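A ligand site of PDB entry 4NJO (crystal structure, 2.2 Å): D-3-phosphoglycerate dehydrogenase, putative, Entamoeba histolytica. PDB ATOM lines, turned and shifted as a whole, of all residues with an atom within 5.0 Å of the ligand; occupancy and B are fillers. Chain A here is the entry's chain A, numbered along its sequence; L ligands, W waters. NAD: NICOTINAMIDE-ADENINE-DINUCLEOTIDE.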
ATOM      1  N   ALA A  80       0.735  -6.575 -22.006  1.00  0.00           N
ATOM      2  CA  ALA A  80       0.702  -6.602 -23.467  1.00  0.00           C
ATOM      3  C   ALA A  80       0.299  -7.972 -24.043  1.00  0.00           C
ATOM      4  O   ALA A  80      -0.688  -8.076 -24.775  1.00  0.00           O
ATOM      5  CB  ALA A  80       2.055  -6.168 -24.016  1.00  0.00           C
ATOM      6  N   GLY A  81       1.087  -9.000 -23.720  1.00  0.00           N
ATOM      7  CA  GLY A  81       0.874 -10.336 -24.283  1.00  0.00           C
ATOM      8  C   GLY A  81      -0.245 -11.084 -23.601  1.00  0.00           C
ATOM      9  O   GLY A  81      -0.450 -10.957 -22.393  1.00  0.00           O
ATOM     10  N   ASP A  83      -0.814 -14.606 -24.529  1.00  0.00           N
ATOM     11  CA  ASP A  83      -0.565 -16.022 -24.831  1.00  0.00           C
ATOM     12  C   ASP A  83      -0.809 -16.934 -23.629  1.00  0.00           C
ATOM     13  O   ASP A  83      -0.946 -18.155 -23.783  1.00  0.00           O
ATOM     14  CB  ASP A  83       0.859 -16.232 -25.369  1.00  0.00           C
ATOM     15  CG  ASP A  83       1.919 -15.630 -24.463  1.00  0.00           C
ATOM     16  OD1 ASP A  83       2.030 -14.376 -24.422  1.00  0.00           O
ATOM     17  OD2 ASP A  83       2.648 -16.394 -23.807  1.00  0.00           O
ATOM     18  N   GLY A 102       0.640  -0.984 -24.245  1.00  0.00           N
ATOM     19  CA  GLY A 102       1.618   0.075 -23.996  1.00  0.00           C
ATOM     20  C   GLY A 102       1.839   0.518 -22.563  1.00  0.00           C
ATOM     21  O   GLY A 102       2.762   1.293 -22.290  1.00  0.00           O
ATOM     22  N   ASN A 104       2.952  -0.980 -19.782  1.00  0.00           N
ATOM     23  CA  ASN A 104       4.229  -1.332 -19.152  1.00  0.00           C
ATOM     24  C   ASN A 104       5.427  -1.207 -20.099  1.00  0.00           C
ATOM     25  O   ASN A 104       6.481  -1.800 -19.848  1.00  0.00           O
ATOM     26  CB  ASN A 104       4.151  -2.737 -18.526  1.00  0.00           C
ATOM     27  CG  ASN A 104       3.869  -3.839 -19.539  1.00  0.00           C
ATOM     28  OD1 ASN A 104       4.047  -3.655 -20.743  1.00  0.00           O
ATOM     29  ND2 ASN A 104       3.443  -5.001 -19.045  1.00  0.00           N
ATOM     30  N   VAL A 108       9.952  -2.401 -19.675  1.00  0.00           N
ATOM     31  CA  VAL A 108      10.590  -3.370 -20.566  1.00  0.00           C
ATOM     32  C   VAL A 108      11.685  -2.719 -21.407  1.00  0.00           C
ATOM     33  O   VAL A 108      12.783  -3.276 -21.535  1.00  0.00           O
ATOM     34  CB  VAL A 108       9.552  -4.025 -21.507  1.00  0.00           C
ATOM     35  CG1 VAL A 108      10.166  -5.207 -22.247  1.00  0.00           C
ATOM     36  CG2 VAL A 108       8.337  -4.475 -20.705  1.00  0.00           C
ATOM     37  N   GLY A 141       9.851  -6.454 -34.409  1.00  0.00           N
ATOM     38  CA  GLY A 141       8.561  -6.120 -33.821  1.00  0.00           C
ATOM     39  C   GLY A 141       8.642  -4.725 -33.207  1.00  0.00           C
ATOM     40  O   GLY A 141       9.215  -4.557 -32.129  1.00  0.00           O
ATOM     41  N   CYS A 142       8.087  -3.741 -33.903  1.00  0.00           N
ATOM     42  CA  CYS A 142       8.196  -2.348 -33.472  1.00  0.00           C
ATOM     43  C   CYS A 142       6.843  -1.772 -33.059  1.00  0.00           C
ATOM     44  O   CYS A 142       6.267  -0.923 -33.746  1.00  0.00           O
ATOM     45  CB  CYS A 142       8.849  -1.490 -34.568  1.00  0.00           C
ATOM     46  SG  CYS A 142       9.470   0.130 -34.033  1.00  0.00           S
ATOM     47  N   GLY A 143       6.339  -2.254 -31.922  1.00  0.00           N
ATOM     48  CA  GLY A 143       5.120  -1.724 -31.313  1.00  0.00           C
ATOM     49  C   GLY A 143       5.482  -0.783 -30.189  1.00  0.00           C
ATOM     50  O   GLY A 143       6.437  -0.025 -30.295  1.00  0.00           O
ATOM     51  N   TYR A 144       4.726  -0.844 -29.095  1.00  0.00           N
ATOM     52  CA  TYR A 144       4.944   0.039 -27.954  1.00  0.00           C
ATOM     53  C   TYR A 144       6.335  -0.073 -27.314  1.00  0.00           C
ATOM     54  O   TYR A 144       7.002   0.952 -27.109  1.00  0.00           O
ATOM     55  CB  TYR A 144       3.855  -0.166 -26.898  1.00  0.00           C
ATOM     56  CG  TYR A 144       2.537   0.495 -27.248  1.00  0.00           C
ATOM     57  CD1 TYR A 144       2.392   1.887 -27.185  1.00  0.00           C
ATOM     58  CD2 TYR A 144       1.431  -0.259 -27.622  1.00  0.00           C
ATOM     59  CE1 TYR A 144       1.195   2.499 -27.499  1.00  0.00           C
ATOM     60  CE2 TYR A 144       0.214   0.341 -27.937  1.00  0.00           C
ATOM     61  CZ  TYR A 144       0.105   1.719 -27.878  1.00  0.00           C
ATOM     62  OH  TYR A 144      -1.091   2.319 -28.184  1.00  0.00           O
ATOM     63  N   VAL A 145       6.771  -1.288 -27.011  1.00  0.00           N
ATOM     64  CA  VAL A 145       8.107  -1.499 -26.443  1.00  0.00           C
ATOM     65  C   VAL A 145       9.187  -1.219 -27.485  1.00  0.00           C
ATOM     66  O   VAL A 145      10.114  -0.442 -27.237  1.00  0.00           O
ATOM     67  CB  VAL A 145       8.284  -2.915 -25.838  1.00  0.00           C
ATOM     68  CG1 VAL A 145       9.707  -3.103 -25.325  1.00  0.00           C
ATOM     69  CG2 VAL A 145       7.290  -3.136 -24.702  1.00  0.00           C
ATOM     70  N   GLY A 146       9.052  -1.840 -28.652  1.00  0.00           N
ATOM     71  CA  GLY A 146       9.993  -1.660 -29.759  1.00  0.00           C
ATOM     72  C   GLY A 146      10.265  -0.202 -30.105  1.00  0.00           C
ATOM     73  O   GLY A 146      11.421   0.186 -30.287  1.00  0.00           O
ATOM     74  N   TYR A 163      12.092  -4.717 -38.574  1.00  0.00           N
ATOM     75  CA  TYR A 163      11.257  -5.753 -39.184  1.00  0.00           C
ATOM     76  C   TYR A 163       9.924  -5.856 -38.432  1.00  0.00           C
ATOM     77  O   TYR A 163       9.886  -6.196 -37.244  1.00  0.00           O
ATOM     78  CB  TYR A 163      11.962  -7.112 -39.208  1.00  0.00           C
ATOM     79  CG  TYR A 163      11.105  -8.230 -39.768  1.00  0.00           C
ATOM     80  CD1 TYR A 163      10.913  -8.382 -41.141  1.00  0.00           C
ATOM     81  CD2 TYR A 163      10.460  -9.135 -38.920  1.00  0.00           C
ATOM     82  CE1 TYR A 163      10.120  -9.391 -41.655  1.00  0.00           C
ATOM     83  CE2 TYR A 163       9.666 -10.151 -39.418  1.00  0.00           C
ATOM     84  CZ  TYR A 163       9.496 -10.279 -40.786  1.00  0.00           C
ATOM     85  OH  TYR A 163       8.707 -11.287 -41.286  1.00  0.00           O
ATOM     86  N   ASP A 164       8.839  -5.568 -39.148  1.00  0.00           N
ATOM     87  CA  ASP A 164       7.477  -5.617 -38.606  1.00  0.00           C
ATOM     88  C   ASP A 164       6.481  -5.470 -39.766  1.00  0.00           C
ATOM     89  O   ASP A 164       6.233  -4.354 -40.234  1.00  0.00           O
ATOM     90  CB  ASP A 164       7.257  -4.514 -37.557  1.00  0.00           C
ATOM     91  CG  ASP A 164       5.964  -4.698 -36.768  1.00  0.00           C
ATOM     92  OD1 ASP A 164       5.909  -4.238 -35.614  1.00  0.00           O
ATOM     93  OD2 ASP A 164       4.996  -5.294 -37.293  1.00  0.00           O
ATOM     94  N   PRO A 165       5.902  -6.603 -40.228  1.00  0.00           N
ATOM     95  CA  PRO A 165       4.976  -6.652 -41.368  1.00  0.00           C
ATOM     96  C   PRO A 165       3.688  -5.854 -41.182  1.00  0.00           C
ATOM     97  O   PRO A 165       3.046  -5.472 -42.167  1.00  0.00           O
ATOM     98  CB  PRO A 165       4.641  -8.148 -41.472  1.00  0.00           C
ATOM     99  CG  PRO A 165       5.770  -8.850 -40.803  1.00  0.00           C
ATOM    100  CD  PRO A 165       6.171  -7.939 -39.684  1.00  0.00           C
ATOM    101  N   PHE A 166       3.296  -5.604 -39.931  1.00  0.00           N
ATOM    102  CA  PHE A 166       2.016  -4.984 -39.614  1.00  0.00           C
ATOM    103  C   PHE A 166       2.039  -3.464 -39.650  1.00  0.00           C
ATOM    104  O   PHE A 166       0.989  -2.817 -39.568  1.00  0.00           O
ATOM    105  CB  PHE A 166       1.504  -5.477 -38.255  1.00  0.00           C
ATOM    106  CG  PHE A 166       1.179  -6.946 -38.213  1.00  0.00           C
ATOM    107  CD1 PHE A 166      -0.146  -7.376 -38.261  1.00  0.00           C
ATOM    108  CD2 PHE A 166       2.185  -7.909 -38.115  1.00  0.00           C
ATOM    109  CE1 PHE A 166      -0.457  -8.731 -38.232  1.00  0.00           C
ATOM    110  CE2 PHE A 166       1.879  -9.256 -38.088  1.00  0.00           C
ATOM    111  CZ  PHE A 166       0.558  -9.667 -38.146  1.00  0.00           C
ATOM    112  N   ILE A 167       3.237  -2.884 -39.770  1.00  0.00           N
ATOM    113  CA  ILE A 167       3.392  -1.422 -39.773  1.00  0.00           C
ATOM    114  C   ILE A 167       4.211  -0.914 -40.957  1.00  0.00           C
ATOM    115  O   ILE A 167       4.870  -1.697 -41.658  1.00  0.00           O
ATOM    116  CB  ILE A 167       4.005  -0.889 -38.456  1.00  0.00           C
ATOM    117  CG1 ILE A 167       5.458  -1.362 -38.287  1.00  0.00           C
ATOM    118  CG2 ILE A 167       3.146  -1.284 -37.243  1.00  0.00           C
ATOM    119  CD1 ILE A 167       6.310  -0.471 -37.417  1.00  0.00           C
ATOM    120  N   HIS A 189      10.730  -8.078 -29.896  1.00  0.00           N
ATOM    121  CA  HIS A 189       9.542  -7.503 -29.278  1.00  0.00           C
ATOM    122  C   HIS A 189       8.269  -8.043 -29.947  1.00  0.00           C
ATOM    123  O   HIS A 189       7.319  -7.303 -30.185  1.00  0.00           O
ATOM    124  CB  HIS A 189       9.586  -5.976 -29.322  1.00  0.00           C
ATOM    125  CG  HIS A 189      10.852  -5.392 -28.767  1.00  0.00           C
ATOM    126  ND1 HIS A 189      11.087  -5.292 -27.421  1.00  0.00           N
ATOM    127  CD2 HIS A 189      11.939  -4.880 -29.385  1.00  0.00           C
ATOM    128  CE1 HIS A 189      12.281  -4.745 -27.221  1.00  0.00           C
ATOM    129  NE2 HIS A 189      12.820  -4.480 -28.402  1.00  0.00           N
ATOM    130  N   LEU A 190       8.287  -9.343 -30.241  1.00  0.00           N
ATOM    131  CA  LEU A 190       7.174 -10.020 -30.905  1.00  0.00           C
ATOM    132  C   LEU A 190       6.286 -10.706 -29.873  1.00  0.00           C
ATOM    133  O   LEU A 190       6.786 -11.206 -28.859  1.00  0.00           O
ATOM    134  CB  LEU A 190       7.693 -11.102 -31.859  1.00  0.00           C
ATOM    135  CG  LEU A 190       8.934 -10.919 -32.727  1.00  0.00           C
ATOM    136  CD1 LEU A 190       9.486 -12.280 -33.133  1.00  0.00           C
ATOM    137  CD2 LEU A 190       8.626 -10.079 -33.953  1.00  0.00           C
ATOM    138  N   PRO A 191       4.965 -10.746 -30.121  1.00  0.00           N
ATOM    139  CA  PRO A 191       4.095 -11.587 -29.295  1.00  0.00           C
ATOM    140  C   PRO A 191       4.265 -13.055 -29.656  1.00  0.00           C
ATOM    141  O   PRO A 191       4.750 -13.368 -30.740  1.00  0.00           O
ATOM    142  CB  PRO A 191       2.683 -11.106 -29.660  1.00  0.00           C
ATOM    143  CG  PRO A 191       2.825 -10.544 -31.035  1.00  0.00           C
ATOM    144  CD  PRO A 191       4.207  -9.970 -31.122  1.00  0.00           C
ATOM    145  N   LEU A 192       3.880 -13.944 -28.736  1.00  0.00           N
ATOM    146  CA  LEU A 192       3.855 -15.378 -29.029  1.00  0.00           C
ATOM    147  C   LEU A 192       2.526 -15.760 -29.688  1.00  0.00           C
ATOM    148  O   LEU A 192       1.476 -15.735 -29.052  1.00  0.00           O
ATOM    149  CB  LEU A 192       4.112 -16.206 -27.756  1.00  0.00           C
ATOM    150  CG  LEU A 192       4.041 -17.742 -27.837  1.00  0.00           C
ATOM    151  CD1 LEU A 192       5.027 -18.314 -28.857  1.00  0.00           C
ATOM    152  CD2 LEU A 192       4.286 -18.365 -26.469  1.00  0.00           C
ATOM    153  N   GLU A 195       2.400 -18.184 -35.497  1.00  0.00           N
ATOM    154  CA  GLU A 195       3.434 -17.765 -36.443  1.00  0.00           C
ATOM    155  C   GLU A 195       4.821 -17.600 -35.820  1.00  0.00           C
ATOM    156  O   GLU A 195       5.815 -18.025 -36.401  1.00  0.00           O
ATOM    157  CB  GLU A 195       2.987 -16.465 -37.138  1.00  0.00           C
ATOM    158  CG  GLU A 195       4.083 -15.714 -37.903  1.00  0.00           C
ATOM    159  CD  GLU A 195       4.599 -16.447 -39.120  1.00  0.00           C
ATOM    160  OE1 GLU A 195       5.785 -16.260 -39.465  1.00  0.00           O
ATOM    161  OE2 GLU A 195       3.820 -17.210 -39.747  1.00  0.00           O
ATOM    162  N   THR A 196       4.876 -17.004 -34.631  1.00  0.00           N
ATOM    163  CA  THR A 196       6.154 -16.624 -34.014  1.00  0.00           C
ATOM    164  C   THR A 196       6.816 -17.719 -33.190  1.00  0.00           C
ATOM    165  O   THR A 196       8.006 -17.620 -32.854  1.00  0.00           O
ATOM    166  CB  THR A 196       6.023 -15.353 -33.151  1.00  0.00           C
ATOM    167  OG1 THR A 196       5.112 -15.588 -32.073  1.00  0.00           O
ATOM    168  CG2 THR A 196       5.527 -14.177 -33.986  1.00  0.00           C
ATOM    169  N   LYS A 199      10.294 -19.285 -34.151  1.00  0.00           N
ATOM    170  CA  LYS A 199      10.694 -18.596 -35.385  1.00  0.00           C
ATOM    171  C   LYS A 199      12.166 -18.190 -35.403  1.00  0.00           C
ATOM    172  O   LYS A 199      12.839 -18.290 -36.434  1.00  0.00           O
ATOM    173  CB  LYS A 199       9.803 -17.378 -35.662  1.00  0.00           C
ATOM    174  CG  LYS A 199       9.912 -16.848 -37.090  1.00  0.00           C
ATOM    175  CD  LYS A 199       9.024 -15.654 -37.351  1.00  0.00           C
ATOM    176  CE  LYS A 199       9.061 -15.278 -38.826  1.00  0.00           C
ATOM    177  NZ  LYS A 199       8.426 -13.956 -39.118  1.00  0.00           N
ATOM    178  N   THR A 217      13.500  -9.661 -24.616  1.00  0.00           N
ATOM    179  CA  THR A 217      12.615  -9.248 -23.516  1.00  0.00           C
ATOM    180  C   THR A 217      11.149  -9.546 -23.861  1.00  0.00           C
ATOM    181  O   THR A 217      10.239  -8.970 -23.252  1.00  0.00           O
ATOM    182  CB  THR A 217      12.780  -7.761 -23.179  1.00  0.00           C
ATOM    183  OG1 THR A 217      12.534  -6.959 -24.349  1.00  0.00           O
ATOM    184  CG2 THR A 217      14.179  -7.473 -22.659  1.00  0.00           C
ATOM    185  N   ALA A 218      10.924 -10.452 -24.810  1.00  0.00           N
ATOM    186  CA  ALA A 218       9.580 -10.786 -25.272  1.00  0.00           C
ATOM    187  C   ALA A 218       9.058 -12.097 -24.666  1.00  0.00           C
ATOM    188  O   ALA A 218       8.445 -12.078 -23.592  1.00  0.00           O
ATOM    189  CB  ALA A 218       9.523 -10.842 -26.797  1.00  0.00           C
ATOM    190  N   ARG A 219       9.282 -13.215 -25.355  1.00  0.00           N
ATOM    191  CA  ARG A 219       8.826 -14.540 -24.922  1.00  0.00           C
ATOM    192  C   ARG A 219       9.873 -15.594 -25.254  1.00  0.00           C
ATOM    193  O   ARG A 219      10.507 -15.523 -26.312  1.00  0.00           O
ATOM    194  CB  ARG A 219       7.498 -14.915 -25.597  1.00  0.00           C
ATOM    195  CG  ARG A 219       6.286 -14.110 -25.145  1.00  0.00           C
ATOM    196  CD  ARG A 219       5.905 -14.416 -23.702  1.00  0.00           C
ATOM    197  NE  ARG A 219       4.688 -13.713 -23.301  1.00  0.00           N
ATOM    198  CZ  ARG A 219       4.664 -12.511 -22.734  1.00  0.00           C
ATOM    199  NH1 ARG A 219       5.796 -11.858 -22.497  1.00  0.00           N
ATOM    200  NH2 ARG A 219       3.507 -11.962 -22.404  1.00  0.00           N
ATOM    201  N   ASP A 243      15.254 -11.681 -20.817  1.00  0.00           N
ATOM    202  CA  ASP A 243      14.421 -11.529 -19.620  1.00  0.00           C
ATOM    203  C   ASP A 243      13.504 -12.743 -19.467  1.00  0.00           C
ATOM    204  O   ASP A 243      12.830 -12.902 -18.457  1.00  0.00           O
ATOM    205  CB  ASP A 243      13.599 -10.226 -19.678  1.00  0.00           C
ATOM    206  CG  ASP A 243      12.867  -9.932 -18.370  1.00  0.00           C
ATOM    207  OD1 ASP A 243      13.396 -10.250 -17.280  1.00  0.00           O
ATOM    208  OD2 ASP A 243      11.745  -9.380 -18.428  1.00  0.00           O
ATOM    209  N   VAL A 244      13.497 -13.609 -20.482  1.00  0.00           N
ATOM    210  CA  VAL A 244      12.675 -14.824 -20.475  1.00  0.00           C
ATOM    211  C   VAL A 244      13.549 -16.074 -20.575  1.00  0.00           C
ATOM    212  O   VAL A 244      13.727 -16.638 -21.660  1.00  0.00           O
ATOM    213  CB  VAL A 244      11.564 -14.788 -21.564  1.00  0.00           C
ATOM    214  CG1 VAL A 244      10.390 -13.942 -21.097  1.00  0.00           C
ATOM    215  CG2 VAL A 244      12.096 -14.260 -22.887  1.00  0.00           C
ATOM    216  N   LYS A 265      11.083 -13.164 -15.124  1.00  0.00           N
ATOM    217  CA  LYS A 265      10.741 -12.065 -16.016  1.00  0.00           C
ATOM    218  C   LYS A 265      10.495 -10.778 -15.203  1.00  0.00           C
ATOM    219  O   LYS A 265       9.526 -10.697 -14.450  1.00  0.00           O
ATOM    220  CB  LYS A 265       9.497 -12.432 -16.834  1.00  0.00           C
ATOM    221  CG  LYS A 265       9.222 -11.517 -18.032  1.00  0.00           C
ATOM    222  CD  LYS A 265       8.073 -12.028 -18.889  1.00  0.00           C
ATOM    223  CE  LYS A 265       6.731 -12.007 -18.164  1.00  0.00           C
ATOM    224  NZ  LYS A 265       6.398 -10.650 -17.641  1.00  0.00           N
ATOM    225  N   ILE A 266      11.391  -9.801 -15.348  1.00  0.00           N
ATOM    226  CA  ILE A 266      11.288  -8.541 -14.576  1.00  0.00           C
ATOM    227  C   ILE A 266      11.033  -7.279 -15.398  1.00  0.00           C
ATOM    228  O   ILE A 266      11.057  -6.170 -14.857  1.00  0.00           O
ATOM    229  CB  ILE A 266      12.517  -8.310 -13.661  1.00  0.00           C
ATOM    230  CG1 ILE A 266      13.824  -8.333 -14.471  1.00  0.00           C
ATOM    231  CG2 ILE A 266      12.536  -9.313 -12.517  1.00  0.00           C
ATOM    232  CD1 ILE A 266      15.008  -7.652 -13.796  1.00  0.00           C
ATOM    233  N   GLY A 267      10.793  -7.437 -16.701  1.00  0.00           N
ATOM    234  CA  GLY A 267      10.501  -6.310 -17.591  1.00  0.00           C
ATOM    235  C   GLY A 267       9.416  -5.386 -17.041  1.00  0.00           C
ATOM    236  O   GLY A 267       9.597  -4.178 -16.984  1.00  0.00           O
ATOM    237  N   ALA A 268       8.294  -5.979 -16.631  1.00  0.00           N
ATOM    238  CA  ALA A 268       7.183  -5.233 -16.060  1.00  0.00           C
ATOM    239  C   ALA A 268       7.219  -5.159 -14.528  1.00  0.00           C
ATOM    240  O   ALA A 268       6.243  -4.731 -13.894  1.00  0.00           O
ATOM    241  CB  ALA A 268       5.855  -5.809 -16.533  1.00  0.00           C
HETATM  242  PA  NAD L   1       2.759  -4.560 -29.182  1.00  0.00           P
HETATM  243  O1A NAD L   1       1.584  -5.348 -29.695  1.00  0.00           O
HETATM  244  O2A NAD L   1       2.613  -3.089 -28.875  1.00  0.00           O
HETATM  245  O5B NAD L   1       3.998  -4.728 -30.198  1.00  0.00           O
HETATM  246  C5B NAD L   1       4.297  -5.997 -30.761  1.00  0.00           C
HETATM  247  C4B NAD L   1       4.702  -5.763 -32.215  1.00  0.00           C
HETATM  248  O4B NAD L   1       5.122  -6.973 -32.839  1.00  0.00           O
HETATM  249  C3B NAD L   1       3.535  -5.217 -33.024  1.00  0.00           C
HETATM  250  O3B NAD L   1       3.853  -3.908 -33.497  1.00  0.00           O
HETATM  251  C2B NAD L   1       3.389  -6.150 -34.195  1.00  0.00           C
HETATM  252  O2B NAD L   1       3.216  -5.456 -35.422  1.00  0.00           O
HETATM  253  C1B NAD L   1       4.695  -6.927 -34.194  1.00  0.00           C
HETATM  254  N9A NAD L   1       4.445  -8.288 -34.720  1.00  0.00           N
HETATM  255  C8A NAD L   1       3.331  -9.002 -34.516  1.00  0.00           C
HETATM  256  N7A NAD L   1       3.411 -10.209 -35.132  1.00  0.00           N
HETATM  257  C5A NAD L   1       4.601 -10.257 -35.764  1.00  0.00           C
HETATM  258  C6A NAD L   1       5.323 -11.233 -36.609  1.00  0.00           C
HETATM  259  N6A NAD L   1       4.773 -12.435 -36.911  1.00  0.00           N
HETATM  260  N1A NAD L   1       6.557 -10.887 -37.065  1.00  0.00           N
HETATM  261  C2A NAD L   1       7.118  -9.693 -36.766  1.00  0.00           C
HETATM  262  N3A NAD L   1       6.515  -8.756 -36.013  1.00  0.00           N
HETATM  263  C4A NAD L   1       5.282  -8.977 -35.484  1.00  0.00           C
HETATM  264  O3  NAD L   1       3.321  -5.301 -27.873  1.00  0.00           O
HETATM  265  PN  NAD L   1       4.449  -4.605 -26.960  1.00  0.00           P
HETATM  266  O1N NAD L   1       3.746  -3.853 -25.858  1.00  0.00           O
HETATM  267  O2N NAD L   1       5.448  -3.886 -27.838  1.00  0.00           O
HETATM  268  O5D NAD L   1       5.156  -5.908 -26.327  1.00  0.00           O
HETATM  269  C5D NAD L   1       5.915  -6.750 -27.187  1.00  0.00           C
HETATM  270  C4D NAD L   1       5.941  -8.196 -26.693  1.00  0.00           C
HETATM  271  O4D NAD L   1       6.920  -8.348 -25.670  1.00  0.00           O
HETATM  272  C3D NAD L   1       4.615  -8.630 -26.085  1.00  0.00           C
HETATM  273  O3D NAD L   1       3.822  -9.261 -27.084  1.00  0.00           O
HETATM  274  C2D NAD L   1       5.006  -9.578 -24.972  1.00  0.00           C
HETATM  275  O2D NAD L   1       5.014 -10.921 -25.463  1.00  0.00           O
HETATM  276  C1D NAD L   1       6.428  -9.185 -24.625  1.00  0.00           C
HETATM  277  N1N NAD L   1       6.441  -8.436 -23.372  1.00  0.00           N
HETATM  278  C2N NAD L   1       7.287  -8.815 -22.399  1.00  0.00           C
HETATM  279  C3N NAD L   1       7.330  -8.115 -21.191  1.00  0.00           C
HETATM  280  C7N NAD L   1       8.278  -8.528 -20.101  1.00  0.00           C
HETATM  281  O7N NAD L   1       8.016  -8.259 -18.935  1.00  0.00           O
HETATM  282  N7N NAD L   1       9.406  -9.158 -20.431  1.00  0.00           N
HETATM  283  C4N NAD L   1       6.488  -7.015 -21.017  1.00  0.00           C
HETATM  284  C5N NAD L   1       5.622  -6.640 -22.043  1.00  0.00           C
HETATM  285  C6N NAD L   1       5.623  -7.376 -23.227  1.00  0.00           C
HETATM  286  O   HOH W   1       2.684 -12.748 -26.556  1.00  0.00           O
HETATM  287  O   HOH W   2       3.582  -2.533 -23.376  1.00  0.00           O
HETATM  288  O   HOH W   3       9.461  -6.642 -25.352  1.00  0.00           O
HETATM  289  O   HOH W   4       7.585  -8.861 -15.838  1.00  0.00           O
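The backbone NH (N) of Gly 143 lies close to an oxygen (O3B) of the ligand, 3.4 Å away.
The side-chain carboxylate (OD2) of Asp 164 is in hydrogen-bond range of an oxygen (O2B) of the ligand.
NZ of Lys 265 lies within hydrogen-bond range of O7N of the ligand, 3.2 Å away.
An oxygen (O2A) of the ligand is in hydrogen-bond range of the backbone NH of Tyr 144 (3.1 Å).
O of Thr 217 lies within hydrogen-bond range of N7N of the ligand, 2.9 Å away.
N of Ala 268 lies within hydrogen-bond range of O7N of the ligand, at 3.3 Å.
The backbone NH of Val 145 lies within hydrogen-bond range of an oxygen (O2N) of the ligand (3.0 Å).
NH1 of Arg 219 lies close to O2D of the ligand, 3.2 Å away.
OD2 of Asp 243 is in hydrogen-bond range of N7N of the ligand.
The backbone NH (N) of Gly 141 sits at hydrogen-bond distance from the backbone carbonyl oxygen (O) of Tyr 163 (2.8 Å).
The side-chain carboxylate (OD1) of Asp 243 sits at hydrogen-bond distance from the backbone NH (N) of Ile 266, 2.8 Å away.
The side-chain carboxylate (OD1) of Asp 164 sits at hydrogen-bond distance from the backbone NH (N) of Cys 142 (2.8 Å).
The backbone NH of Val 108 lies within hydrogen-bond range of the backbone carbonyl oxygen of Gly 267 (3.2 Å).
The backbone carbonyl oxygen of Pro 191 sits at hydrogen-bond distance from the side-chain hydroxyl of Thr 196 (2.6 Å).
The side-chain carboxylate (OD1) of Asp 83 is in salt-bridge range of the guanidinium group (NE) of Arg 219, 3.0 Å away.
The backbone NH of Phe 166 lies within hydrogen-bond range of the side-chain carboxylate of Asp 164, at 3.2 Å.
The side-chain hydroxyl (OH) of Tyr 163 lies within hydrogen-bond range of the side-chain amino group (NZ) of Lys 199 (3.5 Å).
The backbone carbonyl oxygen of His 189 sits close to an oxygen (O4B) of the ligand (3.5 Å).
Residues that only touch the ligand: Val 108, Leu 190, Pro 191, Phe 166, Ala 80, Gly 267, Thr 196, Glu 195, Pro 165, Ala 218, Asn 104, Gly 141, Cys 142 and Tyr 163.
Hydrophobic or aromatic side chains within 4 Å of the ligand: Ala 80, Val 108, Tyr 144, Val 145, Tyr 163, Pro 165, Phe 166, Leu 190, Pro 191 and Ala 218.
24 residues have an atom within 4 Å of the ligand: Ala 80, Asn 104, Val 108, Gly 141, Cys 142, Gly 143, Tyr 144, Val 145, Tyr 163, Asp 164, Pro 165, Phe 166, His 189, Leu 190, Pro 191, Glu 195, Thr 196, Thr 217, Ala 218, Arg 219, Asp 243, Lys 265, Gly 267 and Ala 268.
The nearest printed residue that does not touch the ligand is Lys 199 (4.1 Å).
Water W2 lies within hydrogen-bond range of O1N of the ligand (2.8 Å), OD1 of Asn 104 (2.9 Å) and N of Gly 102 (3.4 Å).
Water W3 lies within hydrogen-bond range of ND1 of His 189 (3.0 Å), O4D of the ligand (3.1 Å) and O of Thr 217 (3.2 Å).
Water W1 lies within hydrogen-bond range of N of Leu 192 (2.8 Å), OD1 of Asp 83 (2.8 Å) and O2D of the ligand (3.2 Å).
Water W4 lies within hydrogen-bond range of the side-chain amino group (NZ) of Lys 265 (2.8 Å), the backbone NH (N) of Ala 268 (3.1 Å) and an oxygen (O7N) of the ligand (3.2 Å).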
